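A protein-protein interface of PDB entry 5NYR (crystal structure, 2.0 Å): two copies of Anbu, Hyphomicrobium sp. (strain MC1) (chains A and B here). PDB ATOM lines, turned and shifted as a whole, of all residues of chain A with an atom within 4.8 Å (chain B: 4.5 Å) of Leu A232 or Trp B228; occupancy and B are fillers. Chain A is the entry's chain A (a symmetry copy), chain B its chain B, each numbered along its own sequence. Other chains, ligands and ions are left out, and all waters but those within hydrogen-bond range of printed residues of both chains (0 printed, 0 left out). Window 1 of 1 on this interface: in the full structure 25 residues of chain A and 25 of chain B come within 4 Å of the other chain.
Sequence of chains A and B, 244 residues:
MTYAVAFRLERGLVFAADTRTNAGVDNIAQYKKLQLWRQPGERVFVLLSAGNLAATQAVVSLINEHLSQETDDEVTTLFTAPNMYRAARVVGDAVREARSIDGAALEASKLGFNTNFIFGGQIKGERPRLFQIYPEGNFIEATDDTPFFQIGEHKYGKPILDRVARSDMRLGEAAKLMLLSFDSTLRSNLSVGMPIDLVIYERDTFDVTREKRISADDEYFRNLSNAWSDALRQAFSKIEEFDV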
ATOM      1  N   ARG A 163      36.105  20.441  17.182  1.00  0.00           N
ATOM      2  CA  ARG A 163      36.167  19.162  17.898  1.00  0.00           C
ATOM      3  C   ARG A 163      36.137  17.930  16.979  1.00  0.00           C
ATOM      4  O   ARG A 163      36.840  16.953  17.242  1.00  0.00           O
ATOM      5  CB  ARG A 163      35.033  19.077  18.928  1.00  0.00           C
ATOM      6  CG  ARG A 163      35.173  20.059  20.083  1.00  0.00           C
ATOM      7  CD  ARG A 163      33.924  20.068  20.953  1.00  0.00           C
ATOM      8  NE  ARG A 163      34.023  20.992  22.086  1.00  0.00           N
ATOM      9  CZ  ARG A 163      34.708  20.772  23.211  1.00  0.00           C
ATOM     10  NH1 ARG A 163      35.398  19.649  23.399  1.00  0.00           N
ATOM     11  NH2 ARG A 163      34.713  21.694  24.171  1.00  0.00           N
ATOM     12  N   TRP A 228      20.899  13.724  13.873  1.00  0.00           N
ATOM     13  CA  TRP A 228      21.809  14.574  14.653  1.00  0.00           C
ATOM     14  C   TRP A 228      21.248  14.949  16.030  1.00  0.00           C
ATOM     15  O   TRP A 228      22.004  15.021  17.000  1.00  0.00           O
ATOM     16  CB  TRP A 228      22.174  15.825  13.842  1.00  0.00           C
ATOM     17  CG  TRP A 228      23.225  16.719  14.448  1.00  0.00           C
ATOM     18  CD1 TRP A 228      23.119  18.061  14.666  1.00  0.00           C
ATOM     19  CD2 TRP A 228      24.537  16.345  14.901  1.00  0.00           C
ATOM     20  NE1 TRP A 228      24.274  18.547  15.223  1.00  0.00           N
ATOM     21  CE2 TRP A 228      25.161  17.517  15.380  1.00  0.00           C
ATOM     22  CE3 TRP A 228      25.244  15.136  14.949  1.00  0.00           C
ATOM     23  CZ2 TRP A 228      26.460  17.517  15.904  1.00  0.00           C
ATOM     24  CZ3 TRP A 228      26.536  15.134  15.471  1.00  0.00           C
ATOM     25  CH2 TRP A 228      27.129  16.319  15.941  1.00  0.00           C
ATOM     26  N   SER A 229      19.937  15.179  16.111  1.00  0.00           N
ATOM     27  CA  SER A 229      19.262  15.402  17.402  1.00  0.00           C
ATOM     28  C   SER A 229      19.378  14.181  18.311  1.00  0.00           C
ATOM     29  O   SER A 229      19.766  14.302  19.475  1.00  0.00           O
ATOM     30  CB  SER A 229      17.783  15.743  17.203  1.00  0.00           C
ATOM     31  OG  SER A 229      17.623  17.026  16.627  1.00  0.00           O
ATOM     32  N   ASP A 230      19.048  13.012  17.763  1.00  0.00           N
ATOM     33  CA  ASP A 230      19.110  11.746  18.506  1.00  0.00           C
ATOM     34  C   ASP A 230      20.537  11.411  18.945  1.00  0.00           C
ATOM     35  O   ASP A 230      20.743  10.935  20.061  1.00  0.00           O
ATOM     36  CB  ASP A 230      18.544  10.591  17.665  1.00  0.00           C
ATOM     37  CG  ASP A 230      17.064  10.760  17.334  1.00  0.00           C
ATOM     38  OD1 ASP A 230      16.318  11.358  18.141  1.00  0.00           O
ATOM     39  OD2 ASP A 230      16.645  10.286  16.259  1.00  0.00           O
ATOM     40  N   ALA A 231      21.508  11.665  18.071  1.00  0.00           N
ATOM     41  CA  ALA A 231      22.921  11.411  18.372  1.00  0.00           C
ATOM     42  C   ALA A 231      23.481  12.383  19.412  1.00  0.00           C
ATOM     43  O   ALA A 231      24.229  11.969  20.297  1.00  0.00           O
ATOM     44  CB  ALA A 231      23.756  11.460  17.101  1.00  0.00           C
ATOM     45  N   LEU A 232      23.129  13.665  19.299  1.00  0.00           N
ATOM     46  CA  LEU A 232      23.516  14.669  20.306  1.00  0.00           C
ATOM     47  C   LEU A 232      22.870  14.388  21.664  1.00  0.00           C
ATOM     48  O   LEU A 232      23.526  14.521  22.699  1.00  0.00           O
ATOM     49  CB  LEU A 232      23.170  16.095  19.851  1.00  0.00           C
ATOM     50  CG  LEU A 232      24.126  16.781  18.872  1.00  0.00           C
ATOM     51  CD1 LEU A 232      23.495  18.064  18.350  1.00  0.00           C
ATOM     52  CD2 LEU A 232      25.470  17.075  19.526  1.00  0.00           C
ATOM     53  N   ARG A 233      21.589  14.010  21.648  1.00  0.00           N
ATOM     54  CA  ARG A 233      20.873  13.603  22.868  1.00  0.00           C
ATOM     55  C   ARG A 233      21.515  12.387  23.525  1.00  0.00           C
ATOM     56  O   ARG A 233      21.742  12.384  24.737  1.00  0.00           O
ATOM     57  CB  ARG A 233      19.401  13.303  22.568  1.00  0.00           C
ATOM     58  CG  ARG A 233      18.542  14.544  22.413  1.00  0.00           C
ATOM     59  CD  ARG A 233      17.211  14.216  21.757  1.00  0.00           C
ATOM     60  NE  ARG A 233      16.482  15.421  21.374  1.00  0.00           N
ATOM     61  CZ  ARG A 233      15.352  15.442  20.665  1.00  0.00           C
ATOM     62  NH1 ARG A 233      14.784  14.313  20.241  1.00  0.00           N
ATOM     63  NH2 ARG A 233      14.781  16.609  20.377  1.00  0.00           N
ATOM     64  N   GLN A 234      21.796  11.361  22.723  1.00  0.00           N
ATOM     65  CA  GLN A 234      22.516  10.178  23.206  1.00  0.00           C
ATOM     66  C   GLN A 234      23.931  10.527  23.671  1.00  0.00           C
ATOM     67  O   GLN A 234      24.392   9.996  24.673  1.00  0.00           O
ATOM     68  CB  GLN A 234      22.563   9.067  22.144  1.00  0.00           C
ATOM     69  CG  GLN A 234      21.275   8.261  22.033  1.00  0.00           C
ATOM     70  CD  GLN A 234      21.443   6.991  21.217  1.00  0.00           C
ATOM     71  OE1 GLN A 234      22.263   6.133  21.547  1.00  0.00           O
ATOM     72  NE2 GLN A 234      20.654   6.857  20.156  1.00  0.00           N
ATOM     73  N   ALA A 235      24.605  11.425  22.948  1.00  0.00           N
ATOM     74  CA  ALA A 235      25.943  11.892  23.329  1.00  0.00           C
ATOM     75  C   ALA A 235      25.923  12.601  24.679  1.00  0.00           C
ATOM     76  O   ALA A 235      26.747  12.303  25.545  1.00  0.00           O
ATOM     77  CB  ALA A 235      26.521  12.810  22.261  1.00  0.00           C
ATOM     78  N   PHE A 236      24.981  13.529  24.854  1.00  0.00           N
ATOM     79  CA  PHE A 236      24.817  14.219  26.137  1.00  0.00           C
ATOM     80  C   PHE A 236      24.279  13.307  27.246  1.00  0.00           C
ATOM     81  O   PHE A 236      24.606  13.506  28.417  1.00  0.00           O
ATOM     82  CB  PHE A 236      23.930  15.463  26.014  1.00  0.00           C
ATOM     83  CG  PHE A 236      23.939  16.314  27.250  1.00  0.00           C
ATOM     84  CD1 PHE A 236      25.054  17.085  27.562  1.00  0.00           C
ATOM     85  CD2 PHE A 236      22.863  16.303  28.134  1.00  0.00           C
ATOM     86  CE1 PHE A 236      25.084  17.854  28.715  1.00  0.00           C
ATOM     87  CE2 PHE A 236      22.887  17.070  29.289  1.00  0.00           C
ATOM     88  CZ  PHE A 236      24.001  17.844  29.579  1.00  0.00           C
ATOM     89  N   SER A 237      23.461  12.318  26.885  1.00  0.00           N
ATOM     90  CA  SER A 237      23.026  11.289  27.841  1.00  0.00           C
ATOM     91  C   SER A 237      24.218  10.522  28.422  1.00  0.00           C
ATOM     92  O   SER A 237      24.217  10.185  29.607  1.00  0.00           O
ATOM     93  CB  SER A 237      22.034  10.313  27.198  1.00  0.00           C
ATOM     94  OG  SER A 237      20.809  10.956  26.894  1.00  0.00           O
ATOM     95  N   ILE A 239      27.314  11.897  28.536  1.00  0.00           N
ATOM     96  CA  ILE A 239      28.011  12.938  29.321  1.00  0.00           C
ATOM     97  C   ILE A 239      27.468  13.029  30.754  1.00  0.00           C
ATOM     98  O   ILE A 239      28.246  13.101  31.709  1.00  0.00           O
ATOM     99  CB  ILE A 239      27.931  14.332  28.634  1.00  0.00           C
ATOM    100  CG1 ILE A 239      28.769  14.355  27.345  1.00  0.00           C
ATOM    101  CG2 ILE A 239      28.368  15.465  29.566  1.00  0.00           C
ATOM    102  CD1 ILE A 239      30.269  14.452  27.543  1.00  0.00           C
ATOM    103  N   ILE B 160      22.459  23.372  19.767  1.00  0.00           N
ATOM    104  CA  ILE B 160      22.669  22.301  20.746  1.00  0.00           C
ATOM    105  C   ILE B 160      21.611  22.379  21.855  1.00  0.00           C
ATOM    106  O   ILE B 160      21.094  21.346  22.285  1.00  0.00           O
ATOM    107  CB  ILE B 160      24.095  22.333  21.364  1.00  0.00           C
ATOM    108  CG1 ILE B 160      25.184  22.234  20.275  1.00  0.00           C
ATOM    109  CG2 ILE B 160      24.279  21.218  22.391  1.00  0.00           C
ATOM    110  CD1 ILE B 160      25.088  21.025  19.365  1.00  0.00           C
ATOM    111  N   ARG B 163      18.086  21.291  20.520  1.00  0.00           N
ATOM    112  CA  ARG B 163      18.003  19.840  20.315  1.00  0.00           C
ATOM    113  C   ARG B 163      17.999  19.024  21.613  1.00  0.00           C
ATOM    114  O   ARG B 163      17.257  18.045  21.720  1.00  0.00           O
ATOM    115  CB  ARG B 163      19.156  19.369  19.418  1.00  0.00           C
ATOM    116  CG  ARG B 163      19.069  19.875  17.986  1.00  0.00           C
ATOM    117  CD  ARG B 163      20.390  19.716  17.249  1.00  0.00           C
ATOM    118  NE  ARG B 163      20.282  20.099  15.842  1.00  0.00           N
ATOM    119  CZ  ARG B 163      19.726  19.359  14.878  1.00  0.00           C
ATOM    120  NH1 ARG B 163      19.204  18.162  15.138  1.00  0.00           N
ATOM    121  NH2 ARG B 163      19.693  19.823  13.631  1.00  0.00           N
ATOM    122  N   VAL B 164      18.820  19.428  22.584  1.00  0.00           N
ATOM    123  CA  VAL B 164      19.104  18.624  23.786  1.00  0.00           C
ATOM    124  C   VAL B 164      18.334  19.061  25.049  1.00  0.00           C
ATOM    125  O   VAL B 164      18.026  18.219  25.898  1.00  0.00           O
ATOM    126  CB  VAL B 164      20.630  18.603  24.077  1.00  0.00           C
ATOM    127  CG1 VAL B 164      20.962  17.730  25.286  1.00  0.00           C
ATOM    128  CG2 VAL B 164      21.401  18.107  22.853  1.00  0.00           C
ATOM    129  N   LEU B 180      28.831  23.601  27.878  1.00  0.00           N
ATOM    130  CA  LEU B 180      29.282  22.847  26.697  1.00  0.00           C
ATOM    131  C   LEU B 180      28.762  23.412  25.372  1.00  0.00           C
ATOM    132  O   LEU B 180      29.497  23.431  24.381  1.00  0.00           O
ATOM    133  CB  LEU B 180      28.901  21.363  26.803  1.00  0.00           C
ATOM    134  CG  LEU B 180      29.696  20.498  27.784  1.00  0.00           C
ATOM    135  CD1 LEU B 180      29.080  19.109  27.863  1.00  0.00           C
ATOM    136  CD2 LEU B 180      31.163  20.411  27.388  1.00  0.00           C
ATOM    137  N   ASP B 183      30.820  26.808  24.876  1.00  0.00           N
ATOM    138  CA  ASP B 183      32.136  26.396  24.379  1.00  0.00           C
ATOM    139  C   ASP B 183      33.037  27.607  24.076  1.00  0.00           C
ATOM    140  O   ASP B 183      33.517  27.788  22.951  1.00  0.00           O
ATOM    141  CB  ASP B 183      31.964  25.477  23.149  1.00  0.00           C
ATOM    142  CG  ASP B 183      32.956  24.321  23.131  1.00  0.00           C
ATOM    143  OD1 ASP B 183      34.106  24.488  23.592  1.00  0.00           O
ATOM    144  OD2 ASP B 183      32.580  23.231  22.650  1.00  0.00           O
ATOM    145  N   LEU B 224      35.442  17.314  31.211  1.00  0.00           N
ATOM    146  CA  LEU B 224      34.124  17.362  30.570  1.00  0.00           C
ATOM    147  C   LEU B 224      34.235  17.724  29.086  1.00  0.00           C
ATOM    148  O   LEU B 224      33.554  17.128  28.250  1.00  0.00           O
ATOM    149  CB  LEU B 224      33.217  18.369  31.289  1.00  0.00           C
ATOM    150  CG  LEU B 224      31.741  18.433  30.878  1.00  0.00           C
ATOM    151  CD1 LEU B 224      31.000  17.171  31.292  1.00  0.00           C
ATOM    152  CD2 LEU B 224      31.078  19.661  31.486  1.00  0.00           C
ATOM    153  N   SER B 225      35.093  18.696  28.774  1.00  0.00           N
ATOM    154  CA  SER B 225      35.335  19.134  27.392  1.00  0.00           C
ATOM    155  C   SER B 225      35.919  18.022  26.517  1.00  0.00           C
ATOM    156  O   SER B 225      35.490  17.846  25.375  1.00  0.00           O
ATOM    157  CB  SER B 225      36.265  20.353  27.371  1.00  0.00           C
ATOM    158  OG  SER B 225      36.483  20.817  26.050  1.00  0.00           O
ATOM    159  N   ASN B 226      36.889  17.282  27.055  1.00  0.00           N
ATOM    160  CA  ASN B 226      37.489  16.139  26.350  1.00  0.00           C
ATOM    161  C   ASN B 226      36.476  15.014  26.120  1.00  0.00           C
ATOM    162  O   ASN B 226      36.480  14.382  25.063  1.00  0.00           O
ATOM    163  CB  ASN B 226      38.700  15.590  27.118  1.00  0.00           C
ATOM    164  CG  ASN B 226      39.852  16.580  27.194  1.00  0.00           C
ATOM    165  OD1 ASN B 226      39.742  17.729  26.761  1.00  0.00           O
ATOM    166  ND2 ASN B 226      40.969  16.135  27.757  1.00  0.00           N
ATOM    167  N   ALA B 227      35.619  14.773  27.111  1.00  0.00           N
ATOM    168  CA  ALA B 227      34.533  13.791  26.997  1.00  0.00           C
ATOM    169  C   ALA B 227      33.472  14.198  25.968  1.00  0.00           C
ATOM    170  O   ALA B 227      32.892  13.339  25.298  1.00  0.00           O
ATOM    171  CB  ALA B 227      33.881  13.566  28.356  1.00  0.00           C
ATOM    172  N   TRP B 228      33.220  15.503  25.862  1.00  0.00           N
ATOM    173  CA  TRP B 228      32.271  16.055  24.889  1.00  0.00           C
ATOM    174  C   TRP B 228      32.771  15.903  23.448  1.00  0.00           C
ATOM    175  O   TRP B 228      31.995  15.530  22.566  1.00  0.00           O
ATOM    176  CB  TRP B 228      31.981  17.524  25.228  1.00  0.00           C
ATOM    177  CG  TRP B 228      30.956  18.221  24.365  1.00  0.00           C
ATOM    178  CD1 TRP B 228      31.124  19.403  23.703  1.00  0.00           C
ATOM    179  CD2 TRP B 228      29.611  17.798  24.093  1.00  0.00           C
ATOM    180  NE1 TRP B 228      29.975  19.741  23.033  1.00  0.00           N
ATOM    181  CE2 TRP B 228      29.029  18.775  23.253  1.00  0.00           C
ATOM    182  CE3 TRP B 228      28.841  16.689  24.473  1.00  0.00           C
ATOM    183  CZ2 TRP B 228      27.711  18.677  22.784  1.00  0.00           C
ATOM    184  CZ3 TRP B 228      27.529  16.590  24.006  1.00  0.00           C
ATOM    185  CH2 TRP B 228      26.979  17.581  23.170  1.00  0.00           C
ATOM    186  N   SER B 229      34.056  16.182  23.218  1.00  0.00           N
ATOM    187  CA  SER B 229      34.690  15.964  21.905  1.00  0.00           C
ATOM    188  C   SER B 229      34.531  14.518  21.440  1.00  0.00           C
ATOM    189  O   SER B 229      34.069  14.267  20.327  1.00  0.00           O
ATOM    190  CB  SER B 229      36.182  16.305  21.949  1.00  0.00           C
ATOM    191  OG  SER B 229      36.395  17.671  22.242  1.00  0.00           O
ATOM    192  N   ASP B 230      34.904  13.582  22.309  1.00  0.00           N
ATOM    193  CA  ASP B 230      34.781  12.146  22.025  1.00  0.00           C
ATOM    194  C   ASP B 230      33.326  11.720  21.815  1.00  0.00           C
ATOM    195  O   ASP B 230      33.037  10.926  20.919  1.00  0.00           O
ATOM    196  CB  ASP B 230      35.411  11.309  23.148  1.00  0.00           C
ATOM    197  CG  ASP B 230      36.926  11.451  23.212  1.00  0.00           C
ATOM    198  OD1 ASP B 230      37.589  11.341  22.157  1.00  0.00           O
ATOM    199  OD2 ASP B 230      37.456  11.659  24.323  1.00  0.00           O
ATOM    200  N   ALA B 231      32.422  12.255  22.636  1.00  0.00           N
ATOM    201  CA  ALA B 231      30.984  11.992  22.501  1.00  0.00           C
ATOM    202  C   ALA B 231      30.410  12.567  21.203  1.00  0.00           C
ATOM    203  O   ALA B 231      29.541  11.950  20.584  1.00  0.00           O
ATOM    204  CB  ALA B 231      30.225  12.538  23.702  1.00  0.00           C
ATOM    205  N   LEU B 232      30.889  13.746  20.804  1.00  0.00           N
ATOM    206  CA  LEU B 232      30.535  14.338  19.505  1.00  0.00           C
ATOM    207  C   LEU B 232      31.107  13.529  18.336  1.00  0.00           C
ATOM    208  O   LEU B 232      30.421  13.330  17.332  1.00  0.00           O
ATOM    209  CB  LEU B 232      31.000  15.800  19.407  1.00  0.00           C
ATOM    210  CG  LEU B 232      30.189  16.855  20.167  1.00  0.00           C
ATOM    211  CD1 LEU B 232      30.957  18.167  20.212  1.00  0.00           C
ATOM    212  CD2 LEU B 232      28.818  17.063  19.538  1.00  0.00           C
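The backbone carbonyl oxygen of Ser B225 sits at hydrogen-bond distance from the guanidinium group of Arg A163. The side-chain carboxylate of Asp B183 is in salt-bridge range of the guanidinium group of Arg A163 (2.7 Å). The side-chain hydroxyl (OG) of Ser B229 lies within hydrogen-bond range of the guanidinium group (NH1) of Arg A163. The guanidinium group (NE) of Arg A233 lies within hydrogen-bond range of the backbone carbonyl oxygen (O) of Arg B163 (2.8 Å). The side-chain hydroxyl of Ser A229 lies within hydrogen-bond range of the guanidinium group of Arg B163 (2.5 Å).
Of the printed residues of chain B, Arg A163 touches Asp B183, Ser B225, Trp B228, Ser B229 and Leu B232. Of the printed residues of chain B, Trp A228 touches Arg B163 (3.6 Å). Leu A232 touches just these residues of chain B: Ile B160 (3.5 Å), Arg B163 (3.7 Å), Trp B228 (3.98 Å) and Leu B232 (3.3 Å). Printed residues of chain B within 4 Å of Arg A233: Arg B163. Of the printed residues of chain A, Ala B231 touches Ala A235 (3.6 Å).
O of Arg A233 lies within hydrogen-bond range of OG of Ser A237, 2.7 Å away. The backbone carbonyl oxygen (O) of Ser B225 sits at hydrogen-bond distance from the side-chain hydroxyl (OG) of Ser B229. OD1 of Asp A230 is in salt-bridge range of NH1 of Arg A233.
Arg A163 touches Trp B228, and with the chains exchanged Trp A228 touches Arg B163. Arg A163 touches Ser B229, and with the chains exchanged Ser A229 touches Arg B163. Leu A232 touches Trp B228, but with the chains exchanged Trp A228 does not touch Leu B232 (4.04 Å). Leu A232 touches its own counterpart, Leu B232. 6 positions are printed for both chains. Of the 17 pairs that touch across the chains among the printed residues, 7 have their exchanged pair printed and touching as well.
Trp B228 touches Arg A163 (CD1 to NE, 3.7 Å). Arg A163 touches Leu B232. CD1 of Trp A228 touches CZ of Arg B163, 3.6 Å away. Ile B160 touches Leu A232 (CD1 to CD1, 3.5 Å). Arg B163 touches Leu A232 (CD to CD1, 3.7 Å). Leu A232 touches Trp B228 (CD2 to CH2, 3.98 Å). CD2 of Leu A232 touches CD2 of Leu B232, at 3.3 Å. Ala A235 touches Ala B231 (CB to O, 3.6 Å). Ile A239 touches Leu B224 (CG2 to CD1, 3.6 Å). Ala B227 touches Ile A239 (C to CD1, 3.6 Å).
Hydrophobic or aromatic side chains of chain A that line the printed part of chain B: Trp A228, Leu A232, Ala A235, Phe A236 and Ile A239. Hydrophobic or aromatic side chains of chain B that line the printed part of chain A: Ile B160, Val B164, Leu B224, Ala B227, Trp B228, Ala B231 and Leu B232. Among the printed residues, 17 pairs touch across the chains.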
